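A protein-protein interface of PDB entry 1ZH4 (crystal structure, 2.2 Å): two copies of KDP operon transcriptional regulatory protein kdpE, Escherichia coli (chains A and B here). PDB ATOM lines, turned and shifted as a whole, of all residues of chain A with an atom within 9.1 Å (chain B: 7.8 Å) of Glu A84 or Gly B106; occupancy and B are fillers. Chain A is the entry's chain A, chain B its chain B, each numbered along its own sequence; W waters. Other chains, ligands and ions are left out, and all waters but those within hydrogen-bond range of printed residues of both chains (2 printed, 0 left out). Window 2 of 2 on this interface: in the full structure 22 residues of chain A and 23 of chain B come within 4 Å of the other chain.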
ATOM      1  N   ARG A  81     -20.762   5.556 -22.176  1.00  0.00           N
ATOM      2  CA  ARG A  81     -20.390   6.158 -20.926  1.00  0.00           C
ATOM      3  C   ARG A  81     -21.311   5.650 -19.834  1.00  0.00           C
ATOM      4  O   ARG A  81     -22.413   6.165 -19.646  1.00  0.00           O
ATOM      5  CB  ARG A  81     -20.525   7.653 -21.045  1.00  0.00           C
ATOM      6  CG  ARG A  81     -19.437   8.284 -21.879  1.00  0.00           C
ATOM      7  CD  ARG A  81     -19.482   9.787 -21.890  1.00  0.00           C
ATOM      8  NE  ARG A  81     -18.789  10.322 -23.070  1.00  0.00           N
ATOM      9  CZ  ARG A  81     -18.625  11.620 -23.313  1.00  0.00           C
ATOM     10  NH1 ARG A  81     -19.103  12.531 -22.469  1.00  0.00           N
ATOM     11  NH2 ARG A  81     -17.987  11.998 -24.410  1.00  0.00           N
ATOM     12  N   SER A  82     -20.879   4.631 -19.109  1.00  0.00           N
ATOM     13  CA  SER A  82     -21.812   3.973 -18.200  1.00  0.00           C
ATOM     14  C   SER A  82     -21.769   4.454 -16.768  1.00  0.00           C
ATOM     15  O   SER A  82     -22.112   3.690 -15.869  1.00  0.00           O
ATOM     16  CB  SER A  82     -21.640   2.464 -18.243  1.00  0.00           C
ATOM     17  OG  SER A  82     -22.859   1.823 -17.876  1.00  0.00           O
ATOM     18  N   GLU A  83     -21.390   5.719 -16.572  1.00  0.00           N
ATOM     19  CA  GLU A  83     -21.118   6.297 -15.246  1.00  0.00           C
ATOM     20  C   GLU A  83     -22.283   7.083 -14.611  1.00  0.00           C
ATOM     21  O   GLU A  83     -22.938   7.880 -15.286  1.00  0.00           O
ATOM     22  CB  GLU A  83     -19.893   7.233 -15.374  1.00  0.00           C
ATOM     23  CG  GLU A  83     -18.545   6.515 -15.395  1.00  0.00           C
ATOM     24  CD  GLU A  83     -18.255   5.780 -14.077  1.00  0.00           C
ATOM     25  OE1 GLU A  83     -18.080   6.492 -13.056  1.00  0.00           O
ATOM     26  OE2 GLU A  83     -18.233   4.513 -14.045  1.00  0.00           O
ATOM     27  N   GLU A  84     -22.516   6.908 -13.311  1.00  0.00           N
ATOM     28  CA  GLU A  84     -23.604   7.640 -12.649  1.00  0.00           C
ATOM     29  C   GLU A  84     -23.607   9.160 -12.925  1.00  0.00           C
ATOM     30  O   GLU A  84     -24.619   9.728 -13.351  1.00  0.00           O
ATOM     31  CB  GLU A  84     -23.666   7.366 -11.145  1.00  0.00           C
ATOM     32  CG  GLU A  84     -24.816   8.111 -10.477  1.00  0.00           C
ATOM     33  CD  GLU A  84     -25.219   7.540  -9.124  1.00  0.00           C
ATOM     34  OE1 GLU A  84     -25.558   6.343  -9.057  1.00  0.00           O
ATOM     35  OE2 GLU A  84     -25.219   8.280  -8.113  1.00  0.00           O
ATOM     36  N   SER A  85     -22.474   9.816 -12.711  1.00  0.00           N
ATOM     37  CA  SER A  85     -22.363  11.254 -12.950  1.00  0.00           C
ATOM     38  C   SER A  85     -22.609  11.603 -14.417  1.00  0.00           C
ATOM     39  O   SER A  85     -23.074  12.704 -14.742  1.00  0.00           O
ATOM     40  CB  SER A  85     -20.966  11.722 -12.568  1.00  0.00           C
ATOM     41  OG  SER A  85     -20.058  11.271 -13.557  1.00  0.00           O
ATOM     42  N   ASP A  86     -22.258  10.679 -15.302  1.00  0.00           N
ATOM     43  CA  ASP A  86     -22.447  10.875 -16.739  1.00  0.00           C
ATOM     44  C   ASP A  86     -23.969  10.887 -17.026  1.00  0.00           C
ATOM     45  O   ASP A  86     -24.475  11.651 -17.849  1.00  0.00           O
ATOM     46  CB  ASP A  86     -21.731   9.758 -17.527  1.00  0.00           C
ATOM     47  CG  ASP A  86     -20.582  10.276 -18.426  1.00  0.00           C
ATOM     48  OD1 ASP A  86     -20.616  11.356 -19.098  1.00  0.00           O
ATOM     49  OD2 ASP A  86     -19.553   9.559 -18.533  1.00  0.00           O
ATOM     50  N   LYS A  87     -24.698  10.044 -16.310  1.00  0.00           N
ATOM     51  CA  LYS A  87     -26.123   9.948 -16.516  1.00  0.00           C
ATOM     52  C   LYS A  87     -26.795  11.205 -15.967  1.00  0.00           C
ATOM     53  O   LYS A  87     -27.667  11.799 -16.629  1.00  0.00           O
ATOM     54  CB  LYS A  87     -26.664   8.674 -15.848  1.00  0.00           C
ATOM     55  CG  LYS A  87     -26.162   7.410 -16.509  1.00  0.00           C
ATOM     56  CD  LYS A  87     -26.783   6.115 -15.919  1.00  0.00           C
ATOM     57  CE  LYS A  87     -26.318   4.872 -16.718  1.00  0.00           C
ATOM     58  NZ  LYS A  87     -26.591   3.547 -16.068  1.00  0.00           N
ATOM     59  N   ILE A  88     -26.387  11.593 -14.759  1.00  0.00           N
ATOM     60  CA  ILE A  88     -26.921  12.774 -14.073  1.00  0.00           C
ATOM     61  C   ILE A  88     -26.669  14.022 -14.909  1.00  0.00           C
ATOM     62  O   ILE A  88     -27.550  14.874 -15.094  1.00  0.00           O
ATOM     63  CB  ILE A  88     -26.258  12.921 -12.718  1.00  0.00           C
ATOM     64  CG1 ILE A  88     -26.803  11.888 -11.760  1.00  0.00           C
ATOM     65  CG2 ILE A  88     -26.545  14.263 -12.125  1.00  0.00           C
ATOM     66  CD1 ILE A  88     -26.177  12.015 -10.404  1.00  0.00           C
ATOM     67  N   ALA A  89     -25.472  14.112 -15.462  1.00  0.00           N
ATOM     68  CA  ALA A  89     -25.155  15.268 -16.285  1.00  0.00           C
ATOM     69  C   ALA A  89     -26.115  15.372 -17.447  1.00  0.00           C
ATOM     70  O   ALA A  89     -26.744  16.400 -17.613  1.00  0.00           O
ATOM     71  CB  ALA A  89     -23.708  15.230 -16.793  1.00  0.00           C
ATOM     72  N   ALA A  90     -26.205  14.305 -18.243  1.00  0.00           N
ATOM     73  CA  ALA A  90     -26.983  14.294 -19.479  1.00  0.00           C
ATOM     74  C   ALA A  90     -28.461  14.542 -19.214  1.00  0.00           C
ATOM     75  O   ALA A  90     -29.134  15.233 -19.995  1.00  0.00           O
ATOM     76  CB  ALA A  90     -26.808  12.995 -20.188  1.00  0.00           C
ATOM     77  N   LEU A  91     -28.955  13.996 -18.105  1.00  0.00           N
ATOM     78  CA  LEU A  91     -30.362  14.135 -17.775  1.00  0.00           C
ATOM     79  C   LEU A  91     -30.670  15.569 -17.382  1.00  0.00           C
ATOM     80  O   LEU A  91     -31.573  16.209 -17.933  1.00  0.00           O
ATOM     81  CB  LEU A  91     -30.745  13.194 -16.643  1.00  0.00           C
ATOM     82  CG  LEU A  91     -31.519  11.929 -17.042  1.00  0.00           C
ATOM     83  CD1 LEU A  91     -31.081  11.392 -18.408  1.00  0.00           C
ATOM     84  CD2 LEU A  91     -31.387  10.863 -15.987  1.00  0.00           C
ATOM     85  N   ASP A  92     -29.890  16.065 -16.428  1.00  0.00           N
ATOM     86  CA  ASP A  92     -29.950  17.463 -16.001  1.00  0.00           C
ATOM     87  C   ASP A  92     -29.783  18.431 -17.159  1.00  0.00           C
ATOM     88  O   ASP A  92     -30.282  19.539 -17.112  1.00  0.00           O
ATOM     89  CB  ASP A  92     -28.901  17.739 -14.925  1.00  0.00           C
ATOM     90  CG  ASP A  92     -29.256  17.096 -13.597  1.00  0.00           C
ATOM     91  OD1 ASP A  92     -30.476  16.999 -13.271  1.00  0.00           O
ATOM     92  OD2 ASP A  92     -28.379  16.649 -12.813  1.00  0.00           O
ATOM     93  N   TYR A  98     -31.883   7.721 -20.663  1.00  0.00           N
ATOM     94  CA  TYR A  98     -30.498   7.378 -20.856  1.00  0.00           C
ATOM     95  C   TYR A  98     -30.320   5.893 -20.764  1.00  0.00           C
ATOM     96  O   TYR A  98     -30.622   5.295 -19.771  1.00  0.00           O
ATOM     97  CB  TYR A  98     -29.655   8.101 -19.800  1.00  0.00           C
ATOM     98  CG  TYR A  98     -28.146   8.102 -20.045  1.00  0.00           C
ATOM     99  CD1 TYR A  98     -27.446   6.914 -20.174  1.00  0.00           C
ATOM    100  CD2 TYR A  98     -27.437   9.292 -20.121  1.00  0.00           C
ATOM    101  CE1 TYR A  98     -26.081   6.899 -20.402  1.00  0.00           C
ATOM    102  CE2 TYR A  98     -26.063   9.299 -20.335  1.00  0.00           C
ATOM    103  CZ  TYR A  98     -25.395   8.094 -20.462  1.00  0.00           C
ATOM    104  OH  TYR A  98     -24.047   8.088 -20.671  1.00  0.00           O
ATOM    105  N   SER A 100     -27.312   2.989 -21.354  1.00  0.00           N
ATOM    106  CA  SER A 100     -25.915   2.661 -21.627  1.00  0.00           C
ATOM    107  C   SER A 100     -25.773   1.507 -22.618  1.00  0.00           C
ATOM    108  O   SER A 100     -26.602   0.600 -22.625  1.00  0.00           O
ATOM    109  CB  SER A 100     -25.188   2.353 -20.308  1.00  0.00           C
ATOM    110  OG  SER A 100     -25.788   1.234 -19.677  1.00  0.00           O
ATOM    111  N   PHE B  16     -34.758   4.988   3.415  1.00  0.00           N
ATOM    112  CA  PHE B  16     -33.701   5.529   2.639  1.00  0.00           C
ATOM    113  C   PHE B  16     -34.234   6.505   1.586  1.00  0.00           C
ATOM    114  O   PHE B  16     -33.643   7.566   1.399  1.00  0.00           O
ATOM    115  CB  PHE B  16     -32.867   4.412   2.034  1.00  0.00           C
ATOM    116  CG  PHE B  16     -31.738   4.906   1.203  1.00  0.00           C
ATOM    117  CD1 PHE B  16     -30.511   5.232   1.793  1.00  0.00           C
ATOM    118  CD2 PHE B  16     -31.885   5.058  -0.178  1.00  0.00           C
ATOM    119  CE1 PHE B  16     -29.431   5.706   0.998  1.00  0.00           C
ATOM    120  CE2 PHE B  16     -30.832   5.525  -0.961  1.00  0.00           C
ATOM    121  CZ  PHE B  16     -29.608   5.850  -0.374  1.00  0.00           C
ATOM    122  N   ALA B  20     -33.695  10.964   1.541  1.00  0.00           N
ATOM    123  CA  ALA B  20     -33.089  11.607   0.387  1.00  0.00           C
ATOM    124  C   ALA B  20     -34.046  12.615  -0.263  1.00  0.00           C
ATOM    125  O   ALA B  20     -33.625  13.666  -0.774  1.00  0.00           O
ATOM    126  CB  ALA B  20     -32.664  10.543  -0.620  1.00  0.00           C
ATOM    127  N   LEU B  99     -35.731   1.638 -12.742  1.00  0.00           N
ATOM    128  CA  LEU B  99     -34.356   1.402 -12.252  1.00  0.00           C
ATOM    129  C   LEU B  99     -34.329   0.087 -11.505  1.00  0.00           C
ATOM    130  O   LEU B  99     -35.201  -0.183 -10.715  1.00  0.00           O
ATOM    131  CB  LEU B  99     -33.897   2.485 -11.279  1.00  0.00           C
ATOM    132  CG  LEU B  99     -33.372   3.833 -11.760  1.00  0.00           C
ATOM    133  CD1 LEU B  99     -32.938   4.671 -10.562  1.00  0.00           C
ATOM    134  CD2 LEU B  99     -32.193   3.714 -12.771  1.00  0.00           C
ATOM    135  N   PHE B 103     -29.387   0.395  -6.766  1.00  0.00           N
ATOM    136  CA  PHE B 103     -29.381   1.592  -7.589  1.00  0.00           C
ATOM    137  C   PHE B 103     -28.514   2.690  -6.955  1.00  0.00           C
ATOM    138  O   PHE B 103     -28.051   2.541  -5.824  1.00  0.00           O
ATOM    139  CB  PHE B 103     -30.809   2.116  -7.745  1.00  0.00           C
ATOM    140  CG  PHE B 103     -31.432   2.569  -6.442  1.00  0.00           C
ATOM    141  CD1 PHE B 103     -31.900   1.637  -5.520  1.00  0.00           C
ATOM    142  CD2 PHE B 103     -31.548   3.912  -6.151  1.00  0.00           C
ATOM    143  CE1 PHE B 103     -32.481   2.047  -4.310  1.00  0.00           C
ATOM    144  CE2 PHE B 103     -32.123   4.343  -4.954  1.00  0.00           C
ATOM    145  CZ  PHE B 103     -32.600   3.412  -4.031  1.00  0.00           C
ATOM    146  N   GLY B 104     -28.291   3.773  -7.703  1.00  0.00           N
ATOM    147  CA  GLY B 104     -27.638   4.950  -7.157  1.00  0.00           C
ATOM    148  C   GLY B 104     -28.679   6.028  -6.887  1.00  0.00           C
ATOM    149  O   GLY B 104     -29.340   6.470  -7.819  1.00  0.00           O
ATOM    150  N   ILE B 105     -28.836   6.453  -5.635  1.00  0.00           N
ATOM    151  CA  ILE B 105     -29.764   7.534  -5.295  1.00  0.00           C
ATOM    152  C   ILE B 105     -29.629   8.732  -6.227  1.00  0.00           C
ATOM    153  O   ILE B 105     -30.619   9.355  -6.601  1.00  0.00           O
ATOM    154  CB  ILE B 105     -29.509   8.020  -3.845  1.00  0.00           C
ATOM    155  CG1 ILE B 105     -30.727   8.773  -3.301  1.00  0.00           C
ATOM    156  CG2 ILE B 105     -28.210   8.936  -3.807  1.00  0.00           C
ATOM    157  CD1 ILE B 105     -32.071   8.057  -3.421  1.00  0.00           C
ATOM    158  N   GLY B 106     -28.382   9.056  -6.570  1.00  0.00           N
ATOM    159  CA  GLY B 106     -28.075  10.114  -7.503  1.00  0.00           C
ATOM    160  C   GLY B 106     -28.820   9.949  -8.817  1.00  0.00           C
ATOM    161  O   GLY B 106     -29.478  10.875  -9.256  1.00  0.00           O
ATOM    162  N   GLU B 107     -28.695   8.786  -9.458  1.00  0.00           N
ATOM    163  CA  GLU B 107     -29.354   8.547 -10.752  1.00  0.00           C
ATOM    164  C   GLU B 107     -30.876   8.673 -10.600  1.00  0.00           C
ATOM    165  O   GLU B 107     -31.521   9.372 -11.375  1.00  0.00           O
ATOM    166  CB  GLU B 107     -28.984   7.184 -11.348  1.00  0.00           C
ATOM    167  CG  GLU B 107     -29.660   6.964 -12.697  1.00  0.00           C
ATOM    168  CD  GLU B 107     -29.286   5.653 -13.366  1.00  0.00           C
ATOM    169  OE1 GLU B 107     -28.536   4.849 -12.759  1.00  0.00           O
ATOM    170  OE2 GLU B 107     -29.768   5.427 -14.504  1.00  0.00           O
ATOM    171  N   LEU B 108     -31.425   8.027  -9.572  1.00  0.00           N
ATOM    172  CA  LEU B 108     -32.828   8.178  -9.226  1.00  0.00           C
ATOM    173  C   LEU B 108     -33.241   9.644  -9.202  1.00  0.00           C
ATOM    174  O   LEU B 108     -34.088  10.078  -9.994  1.00  0.00           O
ATOM    175  CB  LEU B 108     -33.130   7.499  -7.879  1.00  0.00           C
ATOM    176  CG  LEU B 108     -34.569   7.535  -7.348  1.00  0.00           C
ATOM    177  CD1 LEU B 108     -35.564   6.966  -8.384  1.00  0.00           C
ATOM    178  CD2 LEU B 108     -34.723   6.754  -6.052  1.00  0.00           C
ATOM    179  N   GLN B 109     -32.630  10.423  -8.317  1.00  0.00           N
ATOM    180  CA  GLN B 109     -33.129  11.764  -8.051  1.00  0.00           C
ATOM    181  C   GLN B 109     -33.136  12.571  -9.329  1.00  0.00           C
ATOM    182  O   GLN B 109     -34.004  13.415  -9.536  1.00  0.00           O
ATOM    183  CB  GLN B 109     -32.303  12.442  -6.953  1.00  0.00           C
ATOM    184  CG  GLN B 109     -32.839  12.172  -5.538  1.00  0.00           C
ATOM    185  CD  GLN B 109     -32.044  12.911  -4.464  1.00  0.00           C
ATOM    186  OE1 GLN B 109     -30.832  12.769  -4.419  1.00  0.00           O
ATOM    187  NE2 GLN B 109     -32.723  13.705  -3.606  1.00  0.00           N
ATOM    188  N   ALA B 110     -32.173  12.297 -10.197  1.00  0.00           N
ATOM    189  CA  ALA B 110     -32.102  12.977 -11.472  1.00  0.00           C
ATOM    190  C   ALA B 110     -33.290  12.533 -12.351  1.00  0.00           C
ATOM    191  O   ALA B 110     -34.006  13.375 -12.895  1.00  0.00           O
ATOM    192  CB  ALA B 110     -30.791  12.659 -12.164  1.00  0.00           C
ATOM    193  N   ARG B 111     -33.485  11.214 -12.498  1.00  0.00           N
ATOM    194  CA  ARG B 111     -34.641  10.709 -13.225  1.00  0.00           C
ATOM    195  C   ARG B 111     -35.913  11.231 -12.578  1.00  0.00           C
ATOM    196  O   ARG B 111     -36.886  11.537 -13.294  1.00  0.00           O
ATOM    197  CB  ARG B 111     -34.630   9.182 -13.306  1.00  0.00           C
ATOM    198  CG  ARG B 111     -33.424   8.608 -14.075  1.00  0.00           C
ATOM    199  CD  ARG B 111     -33.394   7.070 -14.193  1.00  0.00           C
ATOM    200  NE  ARG B 111     -32.326   6.644 -15.086  1.00  0.00           N
ATOM    201  CZ  ARG B 111     -32.401   6.583 -16.423  1.00  0.00           C
ATOM    202  NH1 ARG B 111     -33.524   6.920 -17.076  1.00  0.00           N
ATOM    203  NH2 ARG B 111     -31.350   6.160 -17.114  1.00  0.00           N
ATOM    204  N   LEU B 112     -35.924  11.363 -11.240  1.00  0.00           N
ATOM    205  CA  LEU B 112     -37.057  12.045 -10.571  1.00  0.00           C
ATOM    206  C   LEU B 112     -37.307  13.457 -11.087  1.00  0.00           C
ATOM    207  O   LEU B 112     -38.456  13.891 -11.255  1.00  0.00           O
ATOM    208  CB  LEU B 112     -36.880  12.130  -9.075  1.00  0.00           C
ATOM    209  CG  LEU B 112     -37.409  10.962  -8.268  1.00  0.00           C
ATOM    210  CD1 LEU B 112     -37.473  11.425  -6.845  1.00  0.00           C
ATOM    211  CD2 LEU B 112     -38.776  10.529  -8.728  1.00  0.00           C
ATOM    212  N   ARG B 113     -36.230  14.171 -11.350  1.00  0.00           N
ATOM    213  CA  ARG B 113     -36.356  15.510 -11.853  1.00  0.00           C
ATOM    214  C   ARG B 113     -36.860  15.528 -13.272  1.00  0.00           C
ATOM    215  O   ARG B 113     -37.645  16.426 -13.630  1.00  0.00           O
ATOM    216  CB  ARG B 113     -35.009  16.221 -11.787  1.00  0.00           C
ATOM    217  CG  ARG B 113     -34.540  16.469 -10.346  1.00  0.00           C
ATOM    218  CD  ARG B 113     -33.425  17.486 -10.262  1.00  0.00           C
ATOM    219  NE  ARG B 113     -32.126  16.905 -10.623  1.00  0.00           N
ATOM    220  CZ  ARG B 113     -31.400  16.125  -9.824  1.00  0.00           C
ATOM    221  NH1 ARG B 113     -31.839  15.782  -8.629  1.00  0.00           N
ATOM    222  NH2 ARG B 113     -30.233  15.665 -10.250  1.00  0.00           N
HETATM  223  O   HOH W   1     -25.606   4.906 -11.945  1.00  0.00           O
HETATM  224  O   HOH W   2     -29.402   3.154 -16.660  1.00  0.00           O
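O of Arg A81 lies within hydrogen-bond range of OH of Tyr A98 (2.7 Å). The guanidinium group (NE) of Arg B111 is in salt-bridge range of the side-chain carboxylate (OE2) of Glu B107. The guanidinium group (NH1) of Arg B113 lies close to the backbone carbonyl oxygen (O) of Gln B109.
No position is printed for both chains. Of the 8 pairs that touch across the chains among the printed residues, none has its exchanged pair printed and touching as well.
Among the printed residues, pairs that only touch across the chains: Glu A84 with Gly B104, Lys A87 with Glu B107, Glu A84 with Gly B106, Leu A91 with Arg B111, Ile A88 with Gly B106 and Glu A84 with Glu B107.
Of the 14 printed residues of chain B, 5 touch a printed residue of chain A. Of the 14 printed residues of chain A, 6 touch a printed residue of chain B. Printed residues of chain A that touch a printed residue of chain B: Glu A84, Lys A87, Ile A88, Leu A91, Asp A92 and Tyr A98. Among the printed residues, Asp or Glu carboxylates within 4 Å of a Lys or Arg side-chain nitrogen of the other chain: Asp A92 with Arg B113.
Glu A84 touches just these residues of chain B: Gly B104 (3.1 Å), Gly B106 (3.4 Å) and Glu B107 (3.7 Å). Printed residues of chain A within 4 Å of Gly B106: Glu A84 and Ile A88. Gly B104 touches just one residue of chain A: Glu A84. No residue of chain A comes within 4 Å of Ile B105. Printed residues of chain B within 4 Å of Leu A91: Arg B111 (3.6 Å). Of the printed residues of chain B, Asp A92 touches Arg B113. Printed residues of chain A within 4 Å of Arg B111: Leu A91 and Tyr A98. Of the printed residues of chain B, Ile A88 touches Gly B106. Glu A83 touches none of the printed residues of chain B. Leu B99 touches none of the printed residues of chain A. The nearest residue of chain B that does not touch Glu A84 is Ile B105 (4.7 Å). The nearest residue of chain A that does not touch Gly B106 is Asp A92 (6.9 Å).
The guanidinium group (NH2) of Arg B111 lies within hydrogen-bond range of the backbone carbonyl oxygen (O) of Tyr A98 (2.9 Å). The side-chain carboxylate of Asp A92 is in salt-bridge range of the guanidinium group of Arg B113 (3.1 Å).
Water W2 bridges NZ of Lys A87 (2.9 Å) and OE2 of Glu B107 (3.2 Å). Water W1 lies within hydrogen-bond range of the side-chain carboxylate (OE1) of Glu B107 (3.0 Å) and the side-chain carboxylate (OE1) of Glu A84 (3.2 Å).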
